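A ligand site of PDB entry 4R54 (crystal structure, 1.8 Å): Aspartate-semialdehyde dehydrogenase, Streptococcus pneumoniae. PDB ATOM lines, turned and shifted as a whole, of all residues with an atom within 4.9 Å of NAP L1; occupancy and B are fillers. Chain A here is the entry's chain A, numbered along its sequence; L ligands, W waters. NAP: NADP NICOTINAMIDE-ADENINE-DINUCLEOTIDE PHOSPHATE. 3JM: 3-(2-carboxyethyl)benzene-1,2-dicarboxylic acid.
The backbone NH of Ser 37 lies within hydrogen-bond range of an oxygen (O2X) of NAP L1 (3.0 Å). An oxygen (O2X) of NAP L1 sits at hydrogen-bond distance from the side-chain hydroxyl (OG) of Ser 37 (2.6 Å). O3B of NAP L1 sits at hydrogen-bond distance from N of Thr 11, 3.5 Å away. OG1 of Thr 11 is in hydrogen-bond range of O1X of NAP L1 (2.6 Å). O7N of NAP L1 lies within hydrogen-bond range of N of Cys 128. SG of Cys 128 lies within hydrogen-bond range of O7N of NAP L1, 3.1 Å away. The guanidinium group (NH2) of Arg 39 is in salt-bridge range of an oxygen (O3X) of NAP L1, 2.6 Å away. The backbone NH of Ser 40 sits close to an oxygen (O2X) of NAP L1, at 3.5 Å. O2X of NAP L1 lies within hydrogen-bond range of OG of Ser 40 (2.7 Å). OG of Ser 71 sits at hydrogen-bond distance from O4D of NAP L1, 2.7 Å away. N of Val 14 sits at hydrogen-bond distance from O2N of NAP L1, at 2.9 Å. N of Ala 13 sits at hydrogen-bond distance from O2A of NAP L1 (2.9 Å). N of Met 162 sits at hydrogen-bond distance from O2A of NAP L1 (2.9 Å). N7N of NAP L1 lies within hydrogen-bond range of O of Pro 126, at 3.0 Å. O of Gly 329 is in hydrogen-bond range of N7N of NAP L1 (3.1 Å). N7N of NAP L1 sits at hydrogen-bond distance from OD1 of Asn 94, at 3.2 Å. The backbone carbonyl oxygen (O) of Gly 9 lies close to an oxygen (O3B) of NAP L1, at 3.5 Å. The backbone NH (N) of Gly 12 sits at hydrogen-bond distance from an oxygen (O3B) of NAP L1, 3.2 Å away. O9 of 3JM L2 lies within salt-bridge range of NH1 of Arg 99. An oxygen (O19) of 3JM L2 lies within hydrogen-bond range of the backbone NH (N) of Ser 74 (2.6 Å). The side-chain hydroxyl of Ser 74 lies within hydrogen-bond range of an oxygen (O12) of 3JM L2 (3.4 Å). N of Ser 96 is in hydrogen-bond range of O12 of 3JM L2 (2.9 Å). An oxygen (O11) of 3JM L2 sits at hydrogen-bond distance from the side-chain hydroxyl of Ser 96.
An oxygen (O2D) of NAP L1 lies within hydrogen-bond range of an oxygen (O12) of 3JM L2 (2.8 Å).
The backbone NH (N) of Arg 39 sits at hydrogen-bond distance from the side-chain hydroxyl (OG) of Ser 37. OG of Ser 71 is in hydrogen-bond range of ND2 of Asn 94 (3.4 Å). The backbone carbonyl oxygen (O) of Ala 36 is in hydrogen-bond range of the side-chain hydroxyl (OG1) of Thr 57, 2.9 Å away. The backbone carbonyl oxygen (O) of Asn 94 lies within hydrogen-bond range of the guanidinium group (NH2) of Arg 99, 3.2 Å away. The side-chain hydroxyl of Thr 76 lies within hydrogen-bond range of the backbone carbonyl oxygen of Ala 72, at 3.2 Å. O of Thr 95 sits at hydrogen-bond distance from NE of Arg 99, 3.2 Å away. The side-chain amide nitrogen (ND2) of Asn 325 sits close to the backbone NH (N) of Gly 159, at 3.2 Å. The side-chain hydroxyl of Ser 158 is in hydrogen-bond range of the side-chain amide nitrogen of Asn 325.
Residues that only touch NAP L1: Ala 36 (3.1 Å), Gly 161 (3.2 Å), Ala 72 (3.2 Å), Thr 95 (3.3 Å), Thr 76 (3.3 Å), Asn 127 (3.5 Å), Thr 57 (3.5 Å), Gly 73 (3.6 Å), Arg 99 (3.6 Å), Ala 10 (3.8 Å), Gly 159 (3.8 Å) and Ser 158 (3.9 Å). Hydrophobic or aromatic side chains within 4 Å of NAP L1: Ala 13, Val 14, Ala 36, Ala 72 and Met 162. Along chain A the residues within 4 Å of NAP L1 span positions 9 to 329.
Water W5 lies within hydrogen-bond range of O2N of NAP L1 (2.4 Å), O of Gly 9 (2.9 Å), N of Gly 15 (3.0 Å), O of Ser 71 (3.2 Å) and N of Gly 12 (3.5 Å). Water W4 bridges a nitrogen (N1A) of NAP L1 (2.8 Å) and the backbone carbonyl oxygen (O) of Thr 57 (2.9 Å). Water W3 bridges the backbone carbonyl oxygen (O) of Gly 159 (2.7 Å) and an oxygen (O1N) of NAP L1 (3.0 Å). Water W7 lies within hydrogen-bond range of the side-chain amide nitrogen (ND2) of Asn 325 (2.7 Å) and the side-chain sulfur (SG) of Cys 128 (3.6 Å).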
ATOM      1  N   GLY A   9      32.667 -14.999  26.165  1.00  0.00           N
ATOM      2  CA  GLY A   9      31.533 -14.782  27.090  1.00  0.00           C
ATOM      3  C   GLY A   9      31.301 -15.988  27.995  1.00  0.00           C
ATOM      4  O   GLY A   9      30.163 -16.458  28.115  1.00  0.00           O
ATOM      5  N   ALA A  10      32.375 -16.486  28.614  1.00  0.00           N
ATOM      6  CA  ALA A  10      32.358 -17.716  29.400  1.00  0.00           C
ATOM      7  C   ALA A  10      31.686 -17.582  30.768  1.00  0.00           C
ATOM      8  O   ALA A  10      31.303 -18.586  31.359  1.00  0.00           O
ATOM      9  CB  ALA A  10      33.773 -18.221  29.583  1.00  0.00           C
ATOM     10  N   THR A  11      31.566 -16.336  31.252  1.00  0.00           N
ATOM     11  CA  THR A  11      31.105 -16.021  32.607  1.00  0.00           C
ATOM     12  C   THR A  11      29.632 -15.721  32.744  1.00  0.00           C
ATOM     13  O   THR A  11      29.147 -15.547  33.855  1.00  0.00           O
ATOM     14  CB  THR A  11      31.832 -14.751  33.122  1.00  0.00           C
ATOM     15  OG1 THR A  11      31.825 -13.744  32.098  1.00  0.00           O
ATOM     16  CG2 THR A  11      33.257 -15.063  33.495  1.00  0.00           C
ATOM     17  N   GLY A  12      28.898 -15.596  31.641  1.00  0.00           N
ATOM     18  CA  GLY A  12      27.486 -15.223  31.716  1.00  0.00           C
ATOM     19  C   GLY A  12      26.559 -16.441  31.788  1.00  0.00           C
ATOM     20  O   GLY A  12      27.002 -17.565  32.021  1.00  0.00           O
ATOM     21  N   ALA A  13      25.276 -16.199  31.589  1.00  0.00           N
ATOM     22  CA  ALA A  13      24.254 -17.227  31.699  1.00  0.00           C
ATOM     23  C   ALA A  13      24.462 -18.308  30.635  1.00  0.00           C
ATOM     24  O   ALA A  13      24.480 -19.491  30.958  1.00  0.00           O
ATOM     25  CB  ALA A  13      22.875 -16.610  31.602  1.00  0.00           C
ATOM     26  N   VAL A  14      24.645 -17.895  29.380  1.00  0.00           N
ATOM     27  CA  VAL A  14      24.874 -18.818  28.291  1.00  0.00           C
ATOM     28  C   VAL A  14      26.230 -19.495  28.457  1.00  0.00           C
ATOM     29  O   VAL A  14      26.351 -20.680  28.245  1.00  0.00           O
ATOM     30  CB  VAL A  14      24.793 -18.143  26.909  1.00  0.00           C
ATOM     31  CG1 VAL A  14      25.223 -19.104  25.804  1.00  0.00           C
ATOM     32  CG2 VAL A  14      23.373 -17.650  26.620  1.00  0.00           C
ATOM     33  N   GLY A  15      27.238 -18.721  28.836  1.00  0.00           N
ATOM     34  CA  GLY A  15      28.571 -19.236  28.955  1.00  0.00           C
ATOM     35  C   GLY A  15      28.724 -20.349  29.960  1.00  0.00           C
ATOM     36  O   GLY A  15      29.488 -21.274  29.731  1.00  0.00           O
ATOM     37  N   ALA A  36      36.219 -13.290  28.141  1.00  0.00           N
ATOM     38  CA  ALA A  36      35.128 -12.453  28.617  1.00  0.00           C
ATOM     39  C   ALA A  36      35.586 -11.002  28.459  1.00  0.00           C
ATOM     40  O   ALA A  36      36.318 -10.695  27.543  1.00  0.00           O
ATOM     41  CB  ALA A  36      34.778 -12.812  30.041  1.00  0.00           C
ATOM     42  N   SER A  37      35.126 -10.097  29.327  1.00  0.00           N
ATOM     43  CA  SER A  37      35.490  -8.690  29.198  1.00  0.00           C
ATOM     44  C   SER A  37      36.685  -8.382  30.078  1.00  0.00           C
ATOM     45  O   SER A  37      37.137  -9.236  30.857  1.00  0.00           O
ATOM     46  CB  SER A  37      34.302  -7.782  29.580  1.00  0.00           C
ATOM     47  OG  SER A  37      34.155  -7.690  30.994  1.00  0.00           O
ATOM     48  N   ARG A  39      36.450  -6.911  32.736  1.00  0.00           N
ATOM     49  CA  ARG A  39      35.964  -7.101  34.109  1.00  0.00           C
ATOM     50  C   ARG A  39      36.295  -8.458  34.724  1.00  0.00           C
ATOM     51  O   ARG A  39      36.695  -8.527  35.877  1.00  0.00           O
ATOM     52  CB  ARG A  39      34.449  -6.867  34.201  1.00  0.00           C
ATOM     53  CG  ARG A  39      34.058  -5.411  33.971  1.00  0.00           C
ATOM     54  CD  ARG A  39      32.549  -5.222  34.054  1.00  0.00           C
ATOM     55  NE  ARG A  39      31.832  -6.016  33.054  1.00  0.00           N
ATOM     56  CZ  ARG A  39      31.763  -5.727  31.759  1.00  0.00           C
ATOM     57  NH1 ARG A  39      32.376  -4.651  31.260  1.00  0.00           N
ATOM     58  NH2 ARG A  39      31.080  -6.519  30.940  1.00  0.00           N
ATOM     59  N   SER A  40      36.124  -9.527  33.951  1.00  0.00           N
ATOM     60  CA  SER A  40      36.402 -10.882  34.432  1.00  0.00           C
ATOM     61  C   SER A  40      37.827 -11.364  34.196  1.00  0.00           C
ATOM     62  O   SER A  40      38.216 -12.386  34.750  1.00  0.00           O
ATOM     63  CB  SER A  40      35.445 -11.899  33.777  1.00  0.00           C
ATOM     64  OG  SER A  40      34.111 -11.504  33.945  1.00  0.00           O
ATOM     65  N   THR A  57      38.752 -10.380  25.818  1.00  0.00           N
ATOM     66  CA  THR A  57      38.585 -10.661  24.407  1.00  0.00           C
ATOM     67  C   THR A  57      39.165  -9.493  23.628  1.00  0.00           C
ATOM     68  O   THR A  57      38.800  -8.348  23.872  1.00  0.00           O
ATOM     69  CB  THR A  57      37.097 -10.866  24.043  1.00  0.00           C
ATOM     70  OG1 THR A  57      36.496 -11.839  24.922  1.00  0.00           O
ATOM     71  CG2 THR A  57      36.954 -11.296  22.619  1.00  0.00           C
ATOM     72  N   SER A  71      29.358 -16.024  22.743  1.00  0.00           N
ATOM     73  CA  SER A  71      28.105 -15.630  23.379  1.00  0.00           C
ATOM     74  C   SER A  71      28.295 -14.482  24.345  1.00  0.00           C
ATOM     75  O   SER A  71      28.015 -14.626  25.542  1.00  0.00           O
ATOM     76  CB  SER A  71      27.458 -16.806  24.084  1.00  0.00           C
ATOM     77  OG  SER A  71      26.190 -16.401  24.570  1.00  0.00           O
ATOM     78  N   ALA A  72      28.730 -13.352  23.804  1.00  0.00           N
ATOM     79  CA  ALA A  72      29.069 -12.194  24.607  1.00  0.00           C
ATOM     80  C   ALA A  72      28.432 -10.914  24.091  1.00  0.00           C
ATOM     81  O   ALA A  72      28.887  -9.810  24.412  1.00  0.00           O
ATOM     82  CB  ALA A  72      30.586 -12.034  24.654  1.00  0.00           C
ATOM     83  N   GLY A  73      27.382 -11.062  23.284  1.00  0.00           N
ATOM     84  CA  GLY A  73      26.626  -9.927  22.771  1.00  0.00           C
ATOM     85  C   GLY A  73      27.012  -9.605  21.343  1.00  0.00           C
ATOM     86  O   GLY A  73      28.139  -9.883  20.930  1.00  0.00           O
ATOM     87  N   SER A  74      26.074  -9.021  20.606  1.00  0.00           N
ATOM     88  CA  SER A  74      26.235  -8.713  19.180  1.00  0.00           C
ATOM     89  C   SER A  74      27.438  -7.852  18.882  1.00  0.00           C
ATOM     90  O   SER A  74      28.169  -8.116  17.931  1.00  0.00           O
ATOM     91  CB  SER A  74      24.986  -8.001  18.649  1.00  0.00           C
ATOM     92  OG  SER A  74      23.982  -8.964  18.382  1.00  0.00           O
ATOM     93  N   THR A  76      30.260  -7.510  20.630  1.00  0.00           N
ATOM     94  CA  THR A  76      31.468  -8.323  20.757  1.00  0.00           C
ATOM     95  C   THR A  76      31.672  -9.248  19.533  1.00  0.00           C
ATOM     96  O   THR A  76      32.782  -9.367  19.027  1.00  0.00           O
ATOM     97  CB  THR A  76      31.439  -9.125  22.083  1.00  0.00           C
ATOM     98  OG1 THR A  76      31.395  -8.214  23.189  1.00  0.00           O
ATOM     99  CG2 THR A  76      32.665 -10.002  22.237  1.00  0.00           C
ATOM    100  N   LYS A  79      32.686  -7.075  16.541  1.00  0.00           N
ATOM    101  CA  LYS A  79      34.054  -6.550  16.649  1.00  0.00           C
ATOM    102  C   LYS A  79      35.148  -7.610  16.522  1.00  0.00           C
ATOM    103  O   LYS A  79      36.214  -7.323  15.948  1.00  0.00           O
ATOM    104  CB  LYS A  79      34.240  -5.786  17.956  1.00  0.00           C
ATOM    105  CG  LYS A  79      33.594  -4.414  17.935  1.00  0.00           C
ATOM    106  CD  LYS A  79      33.884  -3.621  19.206  1.00  0.00           C
ATOM    107  CE  LYS A  79      32.961  -4.058  20.337  1.00  0.00           C
ATOM    108  NZ  LYS A  79      33.391  -3.540  21.665  1.00  0.00           N
ATOM    109  N   TYR A  80      34.903  -8.804  17.056  1.00  0.00           N
ATOM    110  CA  TYR A  80      35.975  -9.777  17.189  1.00  0.00           C
ATOM    111  C   TYR A  80      35.852 -11.049  16.357  1.00  0.00           C
ATOM    112  O   TYR A  80      36.872 -11.653  16.018  1.00  0.00           O
ATOM    113  CB  TYR A  80      36.137 -10.130  18.648  1.00  0.00           C
ATOM    114  CG  TYR A  80      36.511  -8.943  19.510  1.00  0.00           C
ATOM    115  CD1 TYR A  80      37.696  -8.237  19.294  1.00  0.00           C
ATOM    116  CD2 TYR A  80      35.676  -8.510  20.533  1.00  0.00           C
ATOM    117  CE1 TYR A  80      38.036  -7.148  20.075  1.00  0.00           C
ATOM    118  CE2 TYR A  80      36.021  -7.437  21.329  1.00  0.00           C
ATOM    119  CZ  TYR A  80      37.193  -6.757  21.089  1.00  0.00           C
ATOM    120  OH  TYR A  80      37.503  -5.684  21.883  1.00  0.00           O
ATOM    121  N   ASN A  94      26.588 -17.173  18.701  1.00  0.00           N
ATOM    122  CA  ASN A  94      25.296 -17.281  19.322  1.00  0.00           C
ATOM    123  C   ASN A  94      24.470 -15.992  19.296  1.00  0.00           C
ATOM    124  O   ASN A  94      23.339 -15.986  19.781  1.00  0.00           O
ATOM    125  CB  ASN A  94      25.482 -17.775  20.749  1.00  0.00           C
ATOM    126  CG  ASN A  94      24.222 -18.343  21.324  1.00  0.00           C
ATOM    127  OD1 ASN A  94      23.518 -19.109  20.659  1.00  0.00           O
ATOM    128  ND2 ASN A  94      23.899 -17.967  22.562  1.00  0.00           N
ATOM    129  N   THR A  95      24.979 -14.919  18.711  1.00  0.00           N
ATOM    130  CA  THR A  95      24.272 -13.645  18.685  1.00  0.00           C
ATOM    131  C   THR A  95      23.488 -13.460  17.408  1.00  0.00           C
ATOM    132  O   THR A  95      23.638 -14.236  16.460  1.00  0.00           O
ATOM    133  CB  THR A  95      25.222 -12.446  18.794  1.00  0.00           C
ATOM    134  OG1 THR A  95      25.863 -12.206  17.521  1.00  0.00           O
ATOM    135  CG2 THR A  95      26.233 -12.702  19.864  1.00  0.00           C
ATOM    136  N   SER A  96      22.717 -12.378  17.345  1.00  0.00           N
ATOM    137  CA  SER A  96      21.930 -12.063  16.162  1.00  0.00           C
ATOM    138  C   SER A  96      22.740 -11.454  15.015  1.00  0.00           C
ATOM    139  O   SER A  96      22.235 -11.373  13.895  1.00  0.00           O
ATOM    140  CB  SER A  96      20.796 -11.091  16.522  1.00  0.00           C
ATOM    141  OG  SER A  96      21.328  -9.863  17.037  1.00  0.00           O
ATOM    142  N   ARG A  99      23.359 -13.324  11.543  1.00  0.00           N
ATOM    143  CA  ARG A  99      22.331 -14.326  11.167  1.00  0.00           C
ATOM    144  C   ARG A  99      21.738 -14.147   9.778  1.00  0.00           C
ATOM    145  O   ARG A  99      21.354 -15.135   9.151  1.00  0.00           O
ATOM    146  CB  ARG A  99      21.214 -14.349  12.192  1.00  0.00           C
ATOM    147  CG  ARG A  99      21.635 -14.885  13.549  1.00  0.00           C
ATOM    148  CD  ARG A  99      20.451 -14.990  14.454  1.00  0.00           C
ATOM    149  NE  ARG A  99      20.795 -15.547  15.752  1.00  0.00           N
ATOM    150  CZ  ARG A  99      20.258 -15.154  16.906  1.00  0.00           C
ATOM    151  NH1 ARG A  99      19.327 -14.210  16.912  1.00  0.00           N
ATOM    152  NH2 ARG A  99      20.657 -15.708  18.043  1.00  0.00           N
ATOM    153  N   CYS A 125      24.158 -19.473  15.304  1.00  0.00           N
ATOM    154  CA  CYS A 125      23.112 -20.149  16.051  1.00  0.00           C
ATOM    155  C   CYS A 125      21.891 -19.181  16.073  1.00  0.00           C
ATOM    156  O   CYS A 125      22.046 -17.985  16.352  1.00  0.00           O
ATOM    157  CB  CYS A 125      23.662 -20.534  17.442  1.00  0.00           C
ATOM    158  SG  CYS A 125      22.514 -21.191  18.656  1.00  0.00           S
ATOM    159  N   PRO A 126      20.690 -19.669  15.705  1.00  0.00           N
ATOM    160  CA  PRO A 126      19.512 -18.783  15.713  1.00  0.00           C
ATOM    161  C   PRO A 126      19.092 -18.406  17.122  1.00  0.00           C
ATOM    162  O   PRO A 126      19.621 -18.940  18.099  1.00  0.00           O
ATOM    163  CB  PRO A 126      18.409 -19.608  15.029  1.00  0.00           C
ATOM    164  CG  PRO A 126      19.087 -20.813  14.455  1.00  0.00           C
ATOM    165  CD  PRO A 126      20.366 -21.020  15.200  1.00  0.00           C
ATOM    166  N   ASN A 127      18.143 -17.498  17.209  1.00  0.00           N
ATOM    167  CA  ASN A 127      17.468 -17.158  18.463  1.00  0.00           C
ATOM    168  C   ASN A 127      16.770 -18.368  19.094  1.00  0.00           C
ATOM    169  O   ASN A 127      16.197 -19.197  18.375  1.00  0.00           O
ATOM    170  CB  ASN A 127      16.454 -16.046  18.167  1.00  0.00           C
ATOM    171  CG  ASN A 127      15.584 -15.745  19.347  1.00  0.00           C
ATOM    172  OD1 ASN A 127      14.449 -16.194  19.421  1.00  0.00           O
ATOM    173  ND2 ASN A 127      16.125 -15.008  20.320  1.00  0.00           N
ATOM    174  N   CYS A 128      16.806 -18.448  20.430  1.00  0.00           N
ATOM    175  CA  CYS A 128      16.241 -19.569  21.187  1.00  0.00           C
ATOM    176  C   CYS A 128      14.821 -19.909  20.797  1.00  0.00           C
ATOM    177  O   CYS A 128      14.475 -21.087  20.537  1.00  0.00           O
ATOM    178  CB  CYS A 128      16.336 -19.292  22.703  1.00  0.00           C
ATOM    179  SG  CYS A 128      15.969 -17.586  23.187  1.00  0.00           S
ATOM    180  N   ILE A 131      14.674 -21.458  17.472  1.00  0.00           N
ATOM    181  CA  ILE A 131      15.253 -22.800  17.424  1.00  0.00           C
ATOM    182  C   ILE A 131      14.230 -23.862  17.806  1.00  0.00           C
ATOM    183  O   ILE A 131      14.003 -24.798  17.025  1.00  0.00           O
ATOM    184  CB  ILE A 131      16.495 -22.947  18.306  1.00  0.00           C
ATOM    185  CG1 ILE A 131      17.637 -22.080  17.752  1.00  0.00           C
ATOM    186  CG2 ILE A 131      16.951 -24.386  18.360  1.00  0.00           C
ATOM    187  CD1 ILE A 131      18.802 -21.948  18.714  1.00  0.00           C
ATOM    188  N   SER A 158      16.054 -15.824  31.988  1.00  0.00           N
ATOM    189  CA  SER A 158      17.474 -16.171  31.737  1.00  0.00           C
ATOM    190  C   SER A 158      17.918 -15.851  30.323  1.00  0.00           C
ATOM    191  O   SER A 158      19.117 -15.665  30.075  1.00  0.00           O
ATOM    192  CB  SER A 158      17.743 -17.637  32.055  1.00  0.00           C
ATOM    193  OG  SER A 158      16.927 -18.535  31.278  1.00  0.00           O
ATOM    194  N   GLY A 159      16.951 -15.767  29.397  1.00  0.00           N
ATOM    195  CA  GLY A 159      17.201 -15.329  28.047  1.00  0.00           C
ATOM    196  C   GLY A 159      17.752 -13.925  27.950  1.00  0.00           C
ATOM    197  O   GLY A 159      18.402 -13.590  26.975  1.00  0.00           O
ATOM    198  N   ALA A 160      17.524 -13.109  28.979  1.00  0.00           N
ATOM    199  CA  ALA A 160      18.061 -11.760  29.021  1.00  0.00           C
ATOM    200  C   ALA A 160      19.290 -11.620  29.924  1.00  0.00           C
ATOM    201  O   ALA A 160      19.705 -10.500  30.195  1.00  0.00           O
ATOM    202  CB  ALA A 160      16.964 -10.747  29.414  1.00  0.00           C
ATOM    203  N   GLY A 161      19.862 -12.739  30.378  1.00  0.00           N
ATOM    204  CA  GLY A 161      21.170 -12.738  31.056  1.00  0.00           C
ATOM    205  C   GLY A 161      21.183 -12.882  32.570  1.00  0.00           C
ATOM    206  O   GLY A 161      20.135 -12.834  33.234  1.00  0.00           O
ATOM    207  N   MET A 162      22.382 -13.032  33.126  1.00  0.00           N
ATOM    208  CA  MET A 162      22.503 -13.254  34.577  1.00  0.00           C
ATOM    209  C   MET A 162      21.846 -12.113  35.344  1.00  0.00           C
ATOM    210  O   MET A 162      21.216 -12.347  36.367  1.00  0.00           O
ATOM    211  CB  MET A 162      23.957 -13.411  35.014  1.00  0.00           C
ATOM    212  CG  MET A 162      24.508 -14.814  34.870  1.00  0.00           C
ATOM    213  SD  MET A 162      23.672 -16.107  35.830  1.00  0.00           S
ATOM    214  CE  MET A 162      23.064 -15.218  37.255  1.00  0.00           C
ATOM    215  N   ASN A 325      15.862 -22.642  27.180  1.00  0.00           N
ATOM    216  CA  ASN A 325      16.384 -21.624  26.305  1.00  0.00           C
ATOM    217  C   ASN A 325      17.898 -21.439  26.352  1.00  0.00           C
ATOM    218  O   ASN A 325      18.447 -20.796  25.470  1.00  0.00           O
ATOM    219  CB  ASN A 325      15.711 -20.281  26.623  1.00  0.00           C
ATOM    220  CG  ASN A 325      15.937 -19.870  28.054  1.00  0.00           C
ATOM    221  OD1 ASN A 325      15.472 -20.532  28.977  1.00  0.00           O
ATOM    222  ND2 ASN A 325      16.695 -18.788  28.251  1.00  0.00           N
ATOM    223  N   GLY A 329      18.158 -23.821  23.095  1.00  0.00           N
ATOM    224  CA  GLY A 329      17.979 -22.442  22.675  1.00  0.00           C
ATOM    225  C   GLY A 329      19.298 -21.676  22.528  1.00  0.00           C
ATOM    226  O   GLY A 329      19.297 -20.609  21.942  1.00  0.00           O
ATOM    227  N   ALA A 330      20.404 -22.219  23.029  1.00  0.00           N
ATOM    228  CA  ALA A 330      21.701 -21.504  22.934  1.00  0.00           C
ATOM    229  C   ALA A 330      22.924 -22.426  23.000  1.00  0.00           C
ATOM    230  O   ALA A 330      23.485 -22.780  21.953  1.00  0.00           O
ATOM    231  CB  ALA A 330      21.777 -20.402  23.992  1.00  0.00           C
HETATM  232  PA  NAP L   1      25.043 -12.329  30.382  1.00  0.00           P
HETATM  233  O1A NAP L   1      24.851 -10.873  30.738  1.00  0.00           O
HETATM  234  O2A NAP L   1      24.659 -13.389  31.356  1.00  0.00           O
HETATM  235  O5B NAP L   1      26.600 -12.499  29.990  1.00  0.00           O
HETATM  236  C5B NAP L   1      27.264 -11.576  29.157  1.00  0.00           C
HETATM  237  C4B NAP L   1      28.599 -12.220  28.763  1.00  0.00           C
HETATM  238  O4B NAP L   1      29.234 -11.443  27.750  1.00  0.00           O
HETATM  239  C3B NAP L   1      29.577 -12.275  29.925  1.00  0.00           C
HETATM  240  O3B NAP L   1      30.413 -13.410  29.791  1.00  0.00           O
HETATM  241  C2B NAP L   1      30.394 -11.016  29.744  1.00  0.00           C
HETATM  242  O2B NAP L   1      31.682 -11.041  30.353  1.00  0.00           O
HETATM  243  C1B NAP L   1      30.483 -10.983  28.240  1.00  0.00           C
HETATM  244  N9A NAP L   1      30.820  -9.639  27.738  1.00  0.00           N
HETATM  245  C8A NAP L   1      30.138  -8.490  27.899  1.00  0.00           C
HETATM  246  N7A NAP L   1      30.809  -7.477  27.274  1.00  0.00           N
HETATM  247  C5A NAP L   1      31.912  -7.995  26.725  1.00  0.00           C
HETATM  248  C6A NAP L   1      33.055  -7.497  25.945  1.00  0.00           C
HETATM  249  N6A NAP L   1      33.143  -6.199  25.605  1.00  0.00           N
HETATM  250  N1A NAP L   1      33.995  -8.381  25.559  1.00  0.00           N
HETATM  251  C2A NAP L   1      33.928  -9.681  25.878  1.00  0.00           C
HETATM  252  N3A NAP L   1      32.936 -10.206  26.589  1.00  0.00           N
HETATM  253  C4A NAP L   1      31.915  -9.418  27.025  1.00  0.00           C
HETATM  254  O3  NAP L   1      24.332 -12.644  28.976  1.00  0.00           O
HETATM  255  PN  NAP L   1      23.969 -14.123  28.387  1.00  0.00           P
HETATM  256  O1N NAP L   1      22.540 -14.484  28.727  1.00  0.00           O
HETATM  257  O2N NAP L   1      25.033 -15.159  28.655  1.00  0.00           O
HETATM  258  O5D NAP L   1      24.000 -13.805  26.824  1.00  0.00           O
HETATM  259  C5D NAP L   1      25.008 -12.998  26.235  1.00  0.00           C
HETATM  260  C4D NAP L   1      24.735 -12.942  24.742  1.00  0.00           C
HETATM  261  O4D NAP L   1      24.546 -14.256  24.174  1.00  0.00           O
HETATM  262  C3D NAP L   1      23.456 -12.181  24.420  1.00  0.00           C
HETATM  263  O3D NAP L   1      23.616 -10.774  24.488  1.00  0.00           O
HETATM  264  C2D NAP L   1      23.118 -12.745  23.054  1.00  0.00           C
HETATM  265  O2D NAP L   1      23.830 -12.091  22.000  1.00  0.00           O
HETATM  266  C1D NAP L   1      23.557 -14.199  23.145  1.00  0.00           C
HETATM  267  N1N NAP L   1      22.388 -15.027  23.461  1.00  0.00           N
HETATM  268  C2N NAP L   1      21.753 -15.693  22.493  1.00  0.00           C
HETATM  269  C3N NAP L   1      20.647 -16.489  22.783  1.00  0.00           C
HETATM  270  C7N NAP L   1      19.892 -17.251  21.730  1.00  0.00           C
HETATM  271  O7N NAP L   1      18.676 -17.142  21.716  1.00  0.00           O
HETATM  272  N7N NAP L   1      20.528 -18.011  20.841  1.00  0.00           N
HETATM  273  C4N NAP L   1      20.178 -16.573  24.095  1.00  0.00           C
HETATM  274  C5N NAP L   1      20.835 -15.868  25.072  1.00  0.00           C
HETATM  275  C6N NAP L   1      21.936 -15.097  24.736  1.00  0.00           C
HETATM  276  P2B NAP L   1      31.948 -10.276  31.742  1.00  0.00           P
HETATM  277  O1X NAP L   1      31.458 -11.254  32.770  1.00  0.00           O
HETATM  278  O2X NAP L   1      33.444 -10.028  31.763  1.00  0.00           O
HETATM  279  O3X NAP L   1      31.112  -9.042  31.701  1.00  0.00           O
HETATM  280  C7  3JM L   2      18.988 -12.749  22.797  1.00  0.00           C
HETATM  281  O19 3JM L   2      24.432  -7.702  22.190  1.00  0.00           O
HETATM  282  C15 3JM L   2      23.222  -7.708  22.466  1.00  0.00           C
HETATM  283  O16 3JM L   2      22.637  -6.792  23.076  1.00  0.00           O
HETATM  284  C14 3JM L   2      22.450  -8.923  22.018  1.00  0.00           C
HETATM  285  C13 3JM L   2      21.158  -9.052  22.817  1.00  0.00           C
HETATM  286  C4  3JM L   2      20.424 -10.374  22.731  1.00  0.00           C
HETATM  287  C3  3JM L   2      20.329 -11.165  21.562  1.00  0.00           C
HETATM  288  C10 3JM L   2      21.021 -10.763  20.278  1.00  0.00           C
HETATM  289  O12 3JM L   2      22.113 -11.292  19.989  1.00  0.00           O
HETATM  290  O11 3JM L   2      20.549  -9.894  19.526  1.00  0.00           O
HETATM  291  C5  3JM L   2      19.781 -10.770  23.899  1.00  0.00           C
HETATM  292  C6  3JM L   2      19.067 -11.959  23.942  1.00  0.00           C
HETATM  293  C2  3JM L   2      19.612 -12.371  21.608  1.00  0.00           C
HETATM  294  C1  3JM L   2      19.444 -13.290  20.419  1.00  0.00           C
HETATM  295  O8  3JM L   2      19.728 -14.486  20.531  1.00  0.00           O
HETATM  296  O9  3JM L   2      18.972 -12.868  19.338  1.00  0.00           O
HETATM  297  O   HOH W   1      22.209 -10.459  26.967  1.00  0.00           O
HETATM  298  O   HOH W   2      23.717  -9.813  32.696  1.00  0.00           O
HETATM  299  O   HOH W   3      21.007 -12.711  26.916  1.00  0.00           O
HETATM  300  O   HOH W   4      36.670  -7.576  25.679  1.00  0.00           O
HETATM  301  O   HOH W   5      27.401 -15.758  28.490  1.00  0.00           O
HETATM  302  O   HOH W   6      24.133  -9.465  28.686  1.00  0.00           O
HETATM  303  O   HOH W   7      18.094 -17.938  26.049  1.00  0.00           O
